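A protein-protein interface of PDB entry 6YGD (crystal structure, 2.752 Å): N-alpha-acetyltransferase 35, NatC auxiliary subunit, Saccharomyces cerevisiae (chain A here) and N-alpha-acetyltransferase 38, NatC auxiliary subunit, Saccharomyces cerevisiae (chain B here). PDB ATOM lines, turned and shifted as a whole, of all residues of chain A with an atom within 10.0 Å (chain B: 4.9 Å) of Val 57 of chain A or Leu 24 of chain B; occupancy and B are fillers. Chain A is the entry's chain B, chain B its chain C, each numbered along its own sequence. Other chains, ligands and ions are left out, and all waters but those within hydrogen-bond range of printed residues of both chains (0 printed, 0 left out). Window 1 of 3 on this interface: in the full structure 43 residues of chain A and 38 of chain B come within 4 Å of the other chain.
O of Leu 55 of chain A sits at hydrogen-bond distance from N of Ser 57 of chain B, at 2.7 Å.
OG of Ser 57 of chain B is in hydrogen-bond range of OE2 of Glu 56 of chain A (3.4 Å).
The backbone NH (N) of Val 57 of chain A is in hydrogen-bond range of the backbone carbonyl oxygen (O) of Ser 57 of chain B (3.3 Å).
OD1 of Asn 58 of chain A is in hydrogen-bond range of OG of Ser 62 of chain B, 2.5 Å away.
The side-chain carboxylate of Asp 63 of chain A lies within salt-bridge range of the guanidinium group of Arg 22 of chain B, 2.4 Å away.
The guanidinium group (NH1) of Arg 22 of chain B sits at hydrogen-bond distance from the side-chain hydroxyl (OG) of Ser 65 of chain A.
OE2 of Glu 44 of chain B is in hydrogen-bond range of OG of Ser 65 of chain A (2.6 Å).
The side-chain carboxylate of Glu 56 of chain A sits at hydrogen-bond distance from the side-chain amide nitrogen of Asn 59 of chain A (3.0 Å).
N of Ser 65 of chain A is in hydrogen-bond range of OD1 of Asp 63 of chain A (2.8 Å).
O of Val 16 of chain B lies within hydrogen-bond range of N of Leu 24 of chain B, at 2.8 Å.
NH1 of Arg 22 of chain B is in salt-bridge range of OE2 of Glu 44 of chain B (2.6 Å).
N of Leu 39 of chain B lies within hydrogen-bond range of O of Val 56 of chain B, 2.8 Å away.
O of Val 42 of chain B is in hydrogen-bond range of N of Met 53 of chain B.
CG2 of Ile 14 of chain A touches CD1 of Ile 23 of chain B, 3.6 Å away.
Leu 21 of chain A touches Ile 15 of chain B (CD2 to CD1, 3.7 Å).
CD1 of Leu 55 of chain A touches O of Met 53 of chain B (3.7 Å).
O of Leu 55 of chain A touches CA of Val 56 of chain B (3.3 Å).
Val 57 of chain A touches Arg 22 of chain B.
Val 57 of chain A touches Leu 24 of chain B (CG1 to CD1, 3.7 Å).
Val 57 of chain A touches Val 56 of chain B (CG1 to CG1, 3.7 Å).
Val 57 of chain A touches Val 58 of chain B.
CG2 of Val 57 of chain A touches CD of Pro 59 of chain B, 3.6 Å away.
CB of Ser 62 of chain B touches CG2 of Val 57 of chain A (3.8 Å).
Val 57 of chain A touches just these residues of chain B: Arg 22 (3.7 Å), Leu 24 (3.7 Å), Val 56 (3.7 Å), Ser 57 (3.3 Å), Val 58 (3.6 Å), Pro 59 (3.6 Å) and Ser 62 (3.8 Å).
Printed residues of chain A within 4 Å of Leu 24 of chain B: Val 57 (3.7 Å).
No residue of chain A comes within 4 Å of Val 16 of chain B.
Ile 23 of chain B touches one residue of chain A.
No residue of chain A comes within 4 Å of Val 25 of chain B.
Of chain A, only Val 57 comes within 4 Å of Val 58 of chain B.
Of the printed residues of chain A, Ile 15 of chain B touches Leu 21.
Of the printed residues of chain B, Ile 14 of chain A touches Ile 23 (3.6 Å).
Pro 287 of chain A touches none of the printed residues of chain B.
The nearest residue of chain B that does not touch Val 57 of chain A is Leu 18 of chain B (4.3 Å).
The nearest residue of chain A that does not touch Leu 24 of chain B is Ser 65 of chain A (6.6 Å).
Hydrophobic or aromatic side chains of chain A that line the printed part of chain B: Ile 14, Leu 21, Leu 55 and Val 57.
Printed residues of chain B that touch a printed residue of chain A: Ile 15, Arg 22, Ile 23, Leu 24, Glu 44, Met 53, Val 56, Ser 57, Val 58, Pro 59 and Ser 62.
Among the printed residues, Asp or Glu carboxylates within 4 Å of a Lys or Arg side-chain nitrogen of the other chain: Asp 63 of chain A with Arg 22 of chain B (2.4 Å).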
ATOM      1  N   ILE A  14     -22.035   1.431  12.107  1.00  0.00           N
ATOM      2  CA  ILE A  14     -20.887   2.332  12.033  1.00  0.00           C
ATOM      3  C   ILE A  14     -21.353   3.771  11.847  1.00  0.00           C
ATOM      4  O   ILE A  14     -20.868   4.690  12.519  1.00  0.00           O
ATOM      5  CB  ILE A  14     -19.927   1.902  10.907  1.00  0.00           C
ATOM      6  CG1 ILE A  14     -19.008   0.776  11.382  1.00  0.00           C
ATOM      7  CG2 ILE A  14     -19.090   3.080  10.437  1.00  0.00           C
ATOM      8  CD1 ILE A  14     -17.851   0.491  10.442  1.00  0.00           C
ATOM      9  N   THR A  15     -22.304   3.988  10.937  1.00  0.00           N
ATOM     10  CA  THR A  15     -22.806   5.320  10.626  1.00  0.00           C
ATOM     11  C   THR A  15     -24.220   5.537  11.158  1.00  0.00           C
ATOM     12  O   THR A  15     -25.021   6.234  10.533  1.00  0.00           O
ATOM     13  CB  THR A  15     -22.775   5.568   9.119  1.00  0.00           C
ATOM     14  OG1 THR A  15     -23.900   4.926   8.507  1.00  0.00           O
ATOM     15  CG2 THR A  15     -21.496   5.013   8.512  1.00  0.00           C
ATOM     16  N   PHE A  18     -25.268   9.145  11.931  1.00  0.00           N
ATOM     17  CA  PHE A  18     -25.633   9.943  10.769  1.00  0.00           C
ATOM     18  C   PHE A  18     -26.907   9.363  10.167  1.00  0.00           C
ATOM     19  O   PHE A  18     -26.921   8.207   9.730  1.00  0.00           O
ATOM     20  CB  PHE A  18     -24.508   9.960   9.736  1.00  0.00           C
ATOM     21  CG  PHE A  18     -23.172  10.338  10.302  1.00  0.00           C
ATOM     22  CD1 PHE A  18     -22.908  11.645  10.679  1.00  0.00           C
ATOM     23  CD2 PHE A  18     -22.177   9.387  10.451  1.00  0.00           C
ATOM     24  CE1 PHE A  18     -21.675  11.995  11.199  1.00  0.00           C
ATOM     25  CE2 PHE A  18     -20.943   9.731  10.971  1.00  0.00           C
ATOM     26  CZ  PHE A  18     -20.692  11.037  11.346  1.00  0.00           C
ATOM     27  N   LEU A  21     -26.765   9.614   4.658  1.00  0.00           N
ATOM     28  CA  LEU A  21     -25.485   9.877   4.020  1.00  0.00           C
ATOM     29  C   LEU A  21     -25.645   9.830   2.507  1.00  0.00           C
ATOM     30  O   LEU A  21     -26.351   8.968   1.976  1.00  0.00           O
ATOM     31  CB  LEU A  21     -24.429   8.864   4.472  1.00  0.00           C
ATOM     32  CG  LEU A  21     -24.030   8.936   5.947  1.00  0.00           C
ATOM     33  CD1 LEU A  21     -22.996   7.873   6.287  1.00  0.00           C
ATOM     34  CD2 LEU A  21     -23.504  10.321   6.280  1.00  0.00           C
ATOM     35  N   SER A  54       1.016  15.960   9.042  1.00  0.00           N
ATOM     36  CA  SER A  54      -0.090  15.048   8.812  1.00  0.00           C
ATOM     37  C   SER A  54       0.395  13.614   8.650  1.00  0.00           C
ATOM     38  O   SER A  54       1.489  13.356   8.140  1.00  0.00           O
ATOM     39  CB  SER A  54      -0.865  15.465   7.565  1.00  0.00           C
ATOM     40  OG  SER A  54       0.000  15.508   6.445  1.00  0.00           O
ATOM     41  N   LEU A  55      -0.437  12.682   9.103  1.00  0.00           N
ATOM     42  CA  LEU A  55      -0.278  11.270   8.804  1.00  0.00           C
ATOM     43  C   LEU A  55      -0.933  10.977   7.460  1.00  0.00           C
ATOM     44  O   LEU A  55      -1.733  11.764   6.952  1.00  0.00           O
ATOM     45  CB  LEU A  55      -0.903  10.414   9.907  1.00  0.00           C
ATOM     46  CG  LEU A  55      -0.383  10.651  11.331  1.00  0.00           C
ATOM     47  CD1 LEU A  55      -1.312  10.026  12.360  1.00  0.00           C
ATOM     48  CD2 LEU A  55       1.027  10.112  11.498  1.00  0.00           C
ATOM     49  N   GLU A  56      -0.575   9.839   6.870  1.00  0.00           N
ATOM     50  CA  GLU A  56      -1.123   9.460   5.573  1.00  0.00           C
ATOM     51  C   GLU A  56      -1.578   8.008   5.604  1.00  0.00           C
ATOM     52  O   GLU A  56      -0.844   7.134   6.075  1.00  0.00           O
ATOM     53  CB  GLU A  56      -0.096   9.675   4.458  1.00  0.00           C
ATOM     54  CG  GLU A  56      -0.678   9.630   3.054  1.00  0.00           C
ATOM     55  CD  GLU A  56       0.329  10.062   2.011  1.00  0.00           C
ATOM     56  OE1 GLU A  56       1.263   9.282   1.717  1.00  0.00           O
ATOM     57  OE2 GLU A  56       0.203  11.197   1.508  1.00  0.00           O
ATOM     58  N   VAL A  57      -2.790   7.754   5.102  1.00  0.00           N
ATOM     59  CA  VAL A  57      -3.311   6.392   5.072  1.00  0.00           C
ATOM     60  C   VAL A  57      -2.595   5.594   3.992  1.00  0.00           C
ATOM     61  O   VAL A  57      -2.113   6.143   2.992  1.00  0.00           O
ATOM     62  CB  VAL A  57      -4.834   6.375   4.844  1.00  0.00           C
ATOM     63  CG1 VAL A  57      -5.552   7.100   5.969  1.00  0.00           C
ATOM     64  CG2 VAL A  57      -5.178   6.970   3.480  1.00  0.00           C
ATOM     65  N   ASN A  58      -2.528   4.278   4.197  1.00  0.00           N
ATOM     66  CA  ASN A  58      -1.861   3.361   3.272  1.00  0.00           C
ATOM     67  C   ASN A  58      -0.415   3.770   3.021  1.00  0.00           C
ATOM     68  O   ASN A  58       0.141   3.533   1.945  1.00  0.00           O
ATOM     69  CB  ASN A  58      -2.634   3.240   1.959  1.00  0.00           C
ATOM     70  CG  ASN A  58      -3.993   2.611   2.155  1.00  0.00           C
ATOM     71  OD1 ASN A  58      -5.015   3.169   1.755  1.00  0.00           O
ATOM     72  ND2 ASN A  58      -4.014   1.448   2.792  1.00  0.00           N
ATOM     73  N   ASN A  59       0.197   4.396   4.019  1.00  0.00           N
ATOM     74  CA  ASN A  59       1.617   4.723   4.012  1.00  0.00           C
ATOM     75  C   ASN A  59       2.233   3.932   5.155  1.00  0.00           C
ATOM     76  O   ASN A  59       1.947   4.208   6.325  1.00  0.00           O
ATOM     77  CB  ASN A  59       1.845   6.225   4.179  1.00  0.00           C
ATOM     78  CG  ASN A  59       3.240   6.650   3.769  1.00  0.00           C
ATOM     79  OD1 ASN A  59       4.172   5.847   3.774  1.00  0.00           O
ATOM     80  ND2 ASN A  59       3.391   7.918   3.407  1.00  0.00           N
ATOM     81  N   SER A  60       3.060   2.940   4.815  1.00  0.00           N
ATOM     82  CA  SER A  60       3.578   2.018   5.823  1.00  0.00           C
ATOM     83  C   SER A  60       4.322   2.761   6.927  1.00  0.00           C
ATOM     84  O   SER A  60       4.283   2.354   8.095  1.00  0.00           O
ATOM     85  CB  SER A  60       4.487   0.985   5.156  1.00  0.00           C
ATOM     86  OG  SER A  60       4.914  -0.007   6.071  1.00  0.00           O
ATOM     87  N   LYS A  61       4.999   3.857   6.574  1.00  0.00           N
ATOM     88  CA  LYS A  61       5.730   4.650   7.557  1.00  0.00           C
ATOM     89  C   LYS A  61       4.816   5.564   8.368  1.00  0.00           C
ATOM     90  O   LYS A  61       5.181   5.963   9.480  1.00  0.00           O
ATOM     91  CB  LYS A  61       6.810   5.489   6.865  1.00  0.00           C
ATOM     92  CG  LYS A  61       7.864   4.687   6.105  1.00  0.00           C
ATOM     93  CD  LYS A  61       9.132   5.512   5.872  1.00  0.00           C
ATOM     94  CE  LYS A  61       8.909   6.648   4.881  1.00  0.00           C
ATOM     95  NZ  LYS A  61      10.153   7.456   4.715  1.00  0.00           N
ATOM     96  N   LEU A  62       3.634   5.896   7.846  1.00  0.00           N
ATOM     97  CA  LEU A  62       2.784   6.912   8.453  1.00  0.00           C
ATOM     98  C   LEU A  62       1.433   6.401   8.936  1.00  0.00           C
ATOM     99  O   LEU A  62       0.653   7.194   9.473  1.00  0.00           O
ATOM    100  CB  LEU A  62       2.561   8.062   7.465  1.00  0.00           C
ATOM    101  CG  LEU A  62       3.735   8.997   7.186  1.00  0.00           C
ATOM    102  CD1 LEU A  62       3.373   9.974   6.082  1.00  0.00           C
ATOM    103  CD2 LEU A  62       4.127   9.738   8.450  1.00  0.00           C
ATOM    104  N   ASP A  63       1.124   5.117   8.766  1.00  0.00           N
ATOM    105  CA  ASP A  63      -0.180   4.570   9.129  1.00  0.00           C
ATOM    106  C   ASP A  63      -0.030   3.635  10.323  1.00  0.00           C
ATOM    107  O   ASP A  63       0.729   2.663  10.264  1.00  0.00           O
ATOM    108  CB  ASP A  63      -0.815   3.835   7.947  1.00  0.00           C
ATOM    109  CG  ASP A  63      -2.293   3.542   8.158  1.00  0.00           C
ATOM    110  OD1 ASP A  63      -2.754   3.571   9.318  1.00  0.00           O
ATOM    111  OD2 ASP A  63      -2.997   3.277   7.159  1.00  0.00           O
ATOM    112  N   SER A  64      -0.772   3.925  11.395  1.00  0.00           N
ATOM    113  CA  SER A  64      -0.752   3.076  12.580  1.00  0.00           C
ATOM    114  C   SER A  64      -1.592   1.821  12.388  1.00  0.00           C
ATOM    115  O   SER A  64      -1.276   0.772  12.963  1.00  0.00           O
ATOM    116  CB  SER A  64      -1.258   3.856  13.799  1.00  0.00           C
ATOM    117  OG  SER A  64      -0.717   5.166  13.857  1.00  0.00           O
ATOM    118  N   SER A  65      -2.646   1.906  11.569  1.00  0.00           N
ATOM    119  CA  SER A  65      -3.581   0.795  11.414  1.00  0.00           C
ATOM    120  C   SER A  65      -2.963  -0.371  10.651  1.00  0.00           C
ATOM    121  O   SER A  65      -3.283  -1.533  10.930  1.00  0.00           O
ATOM    122  CB  SER A  65      -4.848   1.271  10.702  1.00  0.00           C
ATOM    123  OG  SER A  65      -5.331   2.491  11.239  1.00  0.00           O
ATOM    124  N   LEU A  66      -2.081  -0.087   9.695  1.00  0.00           N
ATOM    125  CA  LEU A  66      -1.472  -1.121   8.867  1.00  0.00           C
ATOM    126  C   LEU A  66      -0.413  -1.937   9.592  1.00  0.00           C
ATOM    127  O   LEU A  66       0.213  -2.796   8.963  1.00  0.00           O
ATOM    128  CB  LEU A  66      -0.852  -0.497   7.615  1.00  0.00           C
ATOM    129  CG  LEU A  66      -1.807   0.177   6.635  1.00  0.00           C
ATOM    130  CD1 LEU A  66      -1.053   0.587   5.384  1.00  0.00           C
ATOM    131  CD2 LEU A  66      -2.950  -0.754   6.300  1.00  0.00           C
ATOM    132  N   PRO A 287       3.607   4.925  13.223  1.00  0.00           N
ATOM    133  CA  PRO A 287       3.959   3.713  13.969  1.00  0.00           C
ATOM    134  C   PRO A 287       5.456   3.643  14.222  1.00  0.00           C
ATOM    135  O   PRO A 287       6.266   4.156  13.444  1.00  0.00           O
ATOM    136  CB  PRO A 287       3.491   2.580  13.049  1.00  0.00           C
ATOM    137  CG  PRO A 287       3.498   3.184  11.686  1.00  0.00           C
ATOM    138  CD  PRO A 287       3.083   4.614  11.883  1.00  0.00           C
ATOM    139  N   LEU B  14     -16.921  15.460   6.866  1.00  0.00           N
ATOM    140  CA  LEU B  14     -17.162  14.529   5.778  1.00  0.00           C
ATOM    141  C   LEU B  14     -16.843  13.116   6.250  1.00  0.00           C
ATOM    142  O   LEU B  14     -16.130  12.914   7.237  1.00  0.00           O
ATOM    143  CB  LEU B  14     -16.320  14.878   4.541  1.00  0.00           C
ATOM    144  CG  LEU B  14     -16.458  16.279   3.946  1.00  0.00           C
ATOM    145  CD1 LEU B  14     -15.460  16.456   2.813  1.00  0.00           C
ATOM    146  CD2 LEU B  14     -17.866  16.519   3.455  1.00  0.00           C
ATOM    147  N   ILE B  15     -17.382  12.134   5.529  1.00  0.00           N
ATOM    148  CA  ILE B  15     -17.165  10.720   5.815  1.00  0.00           C
ATOM    149  C   ILE B  15     -16.454  10.095   4.623  1.00  0.00           C
ATOM    150  O   ILE B  15     -16.941  10.180   3.490  1.00  0.00           O
ATOM    151  CB  ILE B  15     -18.486   9.980   6.107  1.00  0.00           C
ATOM    152  CG1 ILE B  15     -19.181  10.569   7.337  1.00  0.00           C
ATOM    153  CG2 ILE B  15     -18.237   8.490   6.286  1.00  0.00           C
ATOM    154  CD1 ILE B  15     -20.160  11.680   7.019  1.00  0.00           C
ATOM    155  N   VAL B  16     -15.314   9.459   4.880  1.00  0.00           N
ATOM    156  CA  VAL B  16     -14.465   8.897   3.836  1.00  0.00           C
ATOM    157  C   VAL B  16     -14.343   7.397   4.050  1.00  0.00           C
ATOM    158  O   VAL B  16     -13.925   6.949   5.125  1.00  0.00           O
ATOM    159  CB  VAL B  16     -13.075   9.556   3.823  1.00  0.00           C
ATOM    160  CG1 VAL B  16     -12.139   8.786   2.911  1.00  0.00           C
ATOM    161  CG2 VAL B  16     -13.184  11.007   3.382  1.00  0.00           C
ATOM    162  N   LEU B  18     -12.552   3.914   2.995  1.00  0.00           N
ATOM    163  CA  LEU B  18     -11.342   3.389   2.386  1.00  0.00           C
ATOM    164  C   LEU B  18     -11.628   2.030   1.746  1.00  0.00           C
ATOM    165  O   LEU B  18     -12.759   1.537   1.748  1.00  0.00           O
ATOM    166  CB  LEU B  18     -10.220   3.300   3.421  1.00  0.00           C
ATOM    167  CG  LEU B  18      -9.900   4.584   4.199  1.00  0.00           C
ATOM    168  CD1 LEU B  18      -8.791   4.345   5.208  1.00  0.00           C
ATOM    169  CD2 LEU B  18      -9.533   5.729   3.261  1.00  0.00           C
ATOM    170  N   ARG B  22     -12.178  -0.040   7.441  1.00  0.00           N
ATOM    171  CA  ARG B  22     -12.109   1.175   8.238  1.00  0.00           C
ATOM    172  C   ARG B  22     -12.661   2.372   7.473  1.00  0.00           C
ATOM    173  O   ARG B  22     -12.500   2.488   6.255  1.00  0.00           O
ATOM    174  CB  ARG B  22     -10.674   1.444   8.690  1.00  0.00           C
ATOM    175  CG  ARG B  22      -9.652   1.620   7.586  1.00  0.00           C
ATOM    176  CD  ARG B  22      -8.308   2.001   8.189  1.00  0.00           C
ATOM    177  NE  ARG B  22      -7.278   2.235   7.181  1.00  0.00           N
ATOM    178  CZ  ARG B  22      -6.176   2.949   7.393  1.00  0.00           C
ATOM    179  NH1 ARG B  22      -5.964   3.510   8.576  1.00  0.00           N
ATOM    180  NH2 ARG B  22      -5.288   3.113   6.422  1.00  0.00           N
ATOM    181  N   ILE B  23     -13.331   3.254   8.209  1.00  0.00           N
ATOM    182  CA  ILE B  23     -13.935   4.466   7.673  1.00  0.00           C
ATOM    183  C   ILE B  23     -13.400   5.646   8.470  1.00  0.00           C
ATOM    184  O   ILE B  23     -13.269   5.567   9.696  1.00  0.00           O
ATOM    185  CB  ILE B  23     -15.475   4.401   7.747  1.00  0.00           C
ATOM    186  CG1 ILE B  23     -15.976   3.104   7.103  1.00  0.00           C
ATOM    187  CG2 ILE B  23     -16.104   5.620   7.086  1.00  0.00           C
ATOM    188  CD1 ILE B  23     -17.473   2.911   7.170  1.00  0.00           C
ATOM    189  N   LEU B  24     -13.085   6.736   7.777  1.00  0.00           N
ATOM    190  CA  LEU B  24     -12.512   7.922   8.398  1.00  0.00           C
ATOM    191  C   LEU B  24     -13.554   9.027   8.482  1.00  0.00           C
ATOM    192  O   LEU B  24     -14.159   9.393   7.469  1.00  0.00           O
ATOM    193  CB  LEU B  24     -11.293   8.414   7.619  1.00  0.00           C
ATOM    194  CG  LEU B  24     -10.175   7.401   7.386  1.00  0.00           C
ATOM    195  CD1 LEU B  24      -9.051   8.059   6.620  1.00  0.00           C
ATOM    196  CD2 LEU B  24      -9.672   6.823   8.699  1.00  0.00           C
ATOM    197  N   VAL B  25     -13.750   9.560   9.684  1.00  0.00           N
ATOM    198  CA  VAL B  25     -14.653  10.679   9.923  1.00  0.00           C
ATOM    199  C   VAL B  25     -13.805  11.872  10.330  1.00  0.00           C
ATOM    200  O   VAL B  25     -13.113  11.826  11.354  1.00  0.00           O
ATOM    201  CB  VAL B  25     -15.691  10.355  11.009  1.00  0.00           C
ATOM    202  CG1 VAL B  25     -16.672  11.507  11.164  1.00  0.00           C
ATOM    203  CG2 VAL B  25     -16.416   9.060  10.688  1.00  0.00           C
ATOM    204  N   GLY B  26     -13.855  12.938   9.537  1.00  0.00           N
ATOM    205  CA  GLY B  26     -13.061  14.113   9.840  1.00  0.00           C
ATOM    206  C   GLY B  26     -13.576  15.319   9.091  1.00  0.00           C
ATOM    207  O   GLY B  26     -14.528  15.237   8.313  1.00  0.00           O
ATOM    208  N   LEU B  39      -7.755  15.942   6.094  1.00  0.00           N
ATOM    209  CA  LEU B  39      -8.830  15.956   7.075  1.00  0.00           C
ATOM    210  C   LEU B  39      -8.252  16.127   8.471  1.00  0.00           C
ATOM    211  O   LEU B  39      -7.255  15.489   8.820  1.00  0.00           O
ATOM    212  CB  LEU B  39      -9.654  14.661   7.009  1.00  0.00           C
ATOM    213  CG  LEU B  39     -10.136  14.157   5.646  1.00  0.00           C
ATOM    214  CD1 LEU B  39     -10.560  12.701   5.740  1.00  0.00           C
ATOM    215  CD2 LEU B  39     -11.281  15.003   5.123  1.00  0.00           C
ATOM    216  N   VAL B  42      -9.616  13.523  12.679  1.00  0.00           N
ATOM    217  CA  VAL B  42     -10.028  12.294  12.012  1.00  0.00           C
ATOM    218  C   VAL B  42     -10.340  11.221  13.047  1.00  0.00           C
ATOM    219  O   VAL B  42      -9.527  10.935  13.933  1.00  0.00           O
ATOM    220  CB  VAL B  42      -8.941  11.820  11.038  1.00  0.00           C
ATOM    221  CG1 VAL B  42      -9.254  10.421  10.533  1.00  0.00           C
ATOM    222  CG2 VAL B  42      -8.813  12.797   9.883  1.00  0.00           C
ATOM    223  N   GLU B  43     -11.517  10.618  12.925  1.00  0.00           N
ATOM    224  CA  GLU B  43     -11.919   9.479  13.739  1.00  0.00           C
ATOM    225  C   GLU B  43     -11.979   8.253  12.836  1.00  0.00           C
ATOM    226  O   GLU B  43     -12.696   8.254  11.830  1.00  0.00           O
ATOM    227  CB  GLU B  43     -13.270   9.735  14.405  1.00  0.00           C
ATOM    228  CG  GLU B  43     -13.747   8.608  15.301  1.00  0.00           C
ATOM    229  CD  GLU B  43     -15.176   8.801  15.777  1.00  0.00           C
ATOM    230  OE1 GLU B  43     -15.797   9.824  15.418  1.00  0.00           O
ATOM    231  OE2 GLU B  43     -15.680   7.925  16.510  1.00  0.00           O
ATOM    232  N   GLU B  44     -11.213   7.221  13.180  1.00  0.00           N
ATOM    233  CA  GLU B  44     -11.172   5.987  12.406  1.00  0.00           C
ATOM    234  C   GLU B  44     -12.080   4.949  13.047  1.00  0.00           C
ATOM    235  O   GLU B  44     -11.970   4.680  14.247  1.00  0.00           O
ATOM    236  CB  GLU B  44      -9.748   5.441  12.309  1.00  0.00           C
ATOM    237  CG  GLU B  44      -9.672   4.052  11.695  1.00  0.00           C
ATOM    238  CD  GLU B  44      -8.261   3.506  11.659  1.00  0.00           C
ATOM    239  OE1 GLU B  44      -7.873   2.791  12.607  1.00  0.00           O
ATOM    240  OE2 GLU B  44      -7.536   3.802  10.686  1.00  0.00           O
ATOM    241  N   MET B  53      -7.287   9.977  15.246  1.00  0.00           N
ATOM    242  CA  MET B  53      -5.983   9.999  14.590  1.00  0.00           C
ATOM    243  C   MET B  53      -5.462  11.395  14.272  1.00  0.00           C
ATOM    244  O   MET B  53      -4.296  11.510  13.880  1.00  0.00           O
ATOM    245  CB  MET B  53      -6.015   9.167  13.297  1.00  0.00           C
ATOM    246  CG  MET B  53      -6.172   7.668  13.535  1.00  0.00           C
ATOM    247  SD  MET B  53      -5.663   6.641  12.141  1.00  0.00           S
ATOM    248  CE  MET B  53      -6.660   7.327  10.820  1.00  0.00           C
ATOM    249  N   VAL B  56      -4.973  13.853   9.045  1.00  0.00           N
ATOM    250  CA  VAL B  56      -4.635  12.769   8.131  1.00  0.00           C
ATOM    251  C   VAL B  56      -4.867  13.233   6.699  1.00  0.00           C
ATOM    252  O   VAL B  56      -5.826  13.962   6.418  1.00  0.00           O
ATOM    253  CB  VAL B  56      -5.462  11.498   8.428  1.00  0.00           C
ATOM    254  CG1 VAL B  56      -4.965  10.327   7.593  1.00  0.00           C
ATOM    255  CG2 VAL B  56      -5.417  11.157   9.910  1.00  0.00           C
ATOM    256  N   SER B  57      -3.986  12.817   5.795  1.00  0.00           N
ATOM    257  CA  SER B  57      -4.159  13.034   4.366  1.00  0.00           C
ATOM    258  C   SER B  57      -4.385  11.688   3.693  1.00  0.00           C
ATOM    259  O   SER B  57      -3.656  10.728   3.966  1.00  0.00           O
ATOM    260  CB  SER B  57      -2.939  13.728   3.759  1.00  0.00           C
ATOM    261  OG  SER B  57      -1.873  12.809   3.591  1.00  0.00           O
ATOM    262  N   VAL B  58      -5.385  11.615   2.821  1.00  0.00           N
ATOM    263  CA  VAL B  58      -5.755  10.373   2.154  1.00  0.00           C
ATOM    264  C   VAL B  58      -5.521  10.526   0.654  1.00  0.00           C
ATOM    265  O   VAL B  58      -6.018  11.472   0.037  1.00  0.00           O
ATOM    266  CB  VAL B  58      -7.204   9.955   2.454  1.00  0.00           C
ATOM    267  CG1 VAL B  58      -7.392   9.808   3.956  1.00  0.00           C
ATOM    268  CG2 VAL B  58      -8.218  10.947   1.894  1.00  0.00           C
ATOM    269  N   PRO B  59      -4.733   9.653   0.035  1.00  0.00           N
ATOM    270  CA  PRO B  59      -4.555   9.714  -1.417  1.00  0.00           C
ATOM    271  C   PRO B  59      -5.833   9.322  -2.141  1.00  0.00           C
ATOM    272  O   PRO B  59      -6.732   8.697  -1.577  1.00  0.00           O
ATOM    273  CB  PRO B  59      -3.431   8.704  -1.677  1.00  0.00           C
ATOM    274  CG  PRO B  59      -2.719   8.588  -0.357  1.00  0.00           C
ATOM    275  CD  PRO B  59      -3.795   8.716   0.671  1.00  0.00           C
ATOM    276  N   SER B  62      -6.733   5.631  -2.254  1.00  0.00           N
ATOM    277  CA  SER B  62      -7.225   5.059  -1.008  1.00  0.00           C
ATOM    278  C   SER B  62      -8.701   5.343  -0.773  1.00  0.00           C
ATOM    279  O   SER B  62      -9.328   4.654   0.037  1.00  0.00           O
ATOM    280  CB  SER B  62      -6.404   5.585   0.171  1.00  0.00           C
ATOM    281  OG  SER B  62      -5.079   5.084   0.120  1.00  0.00           O
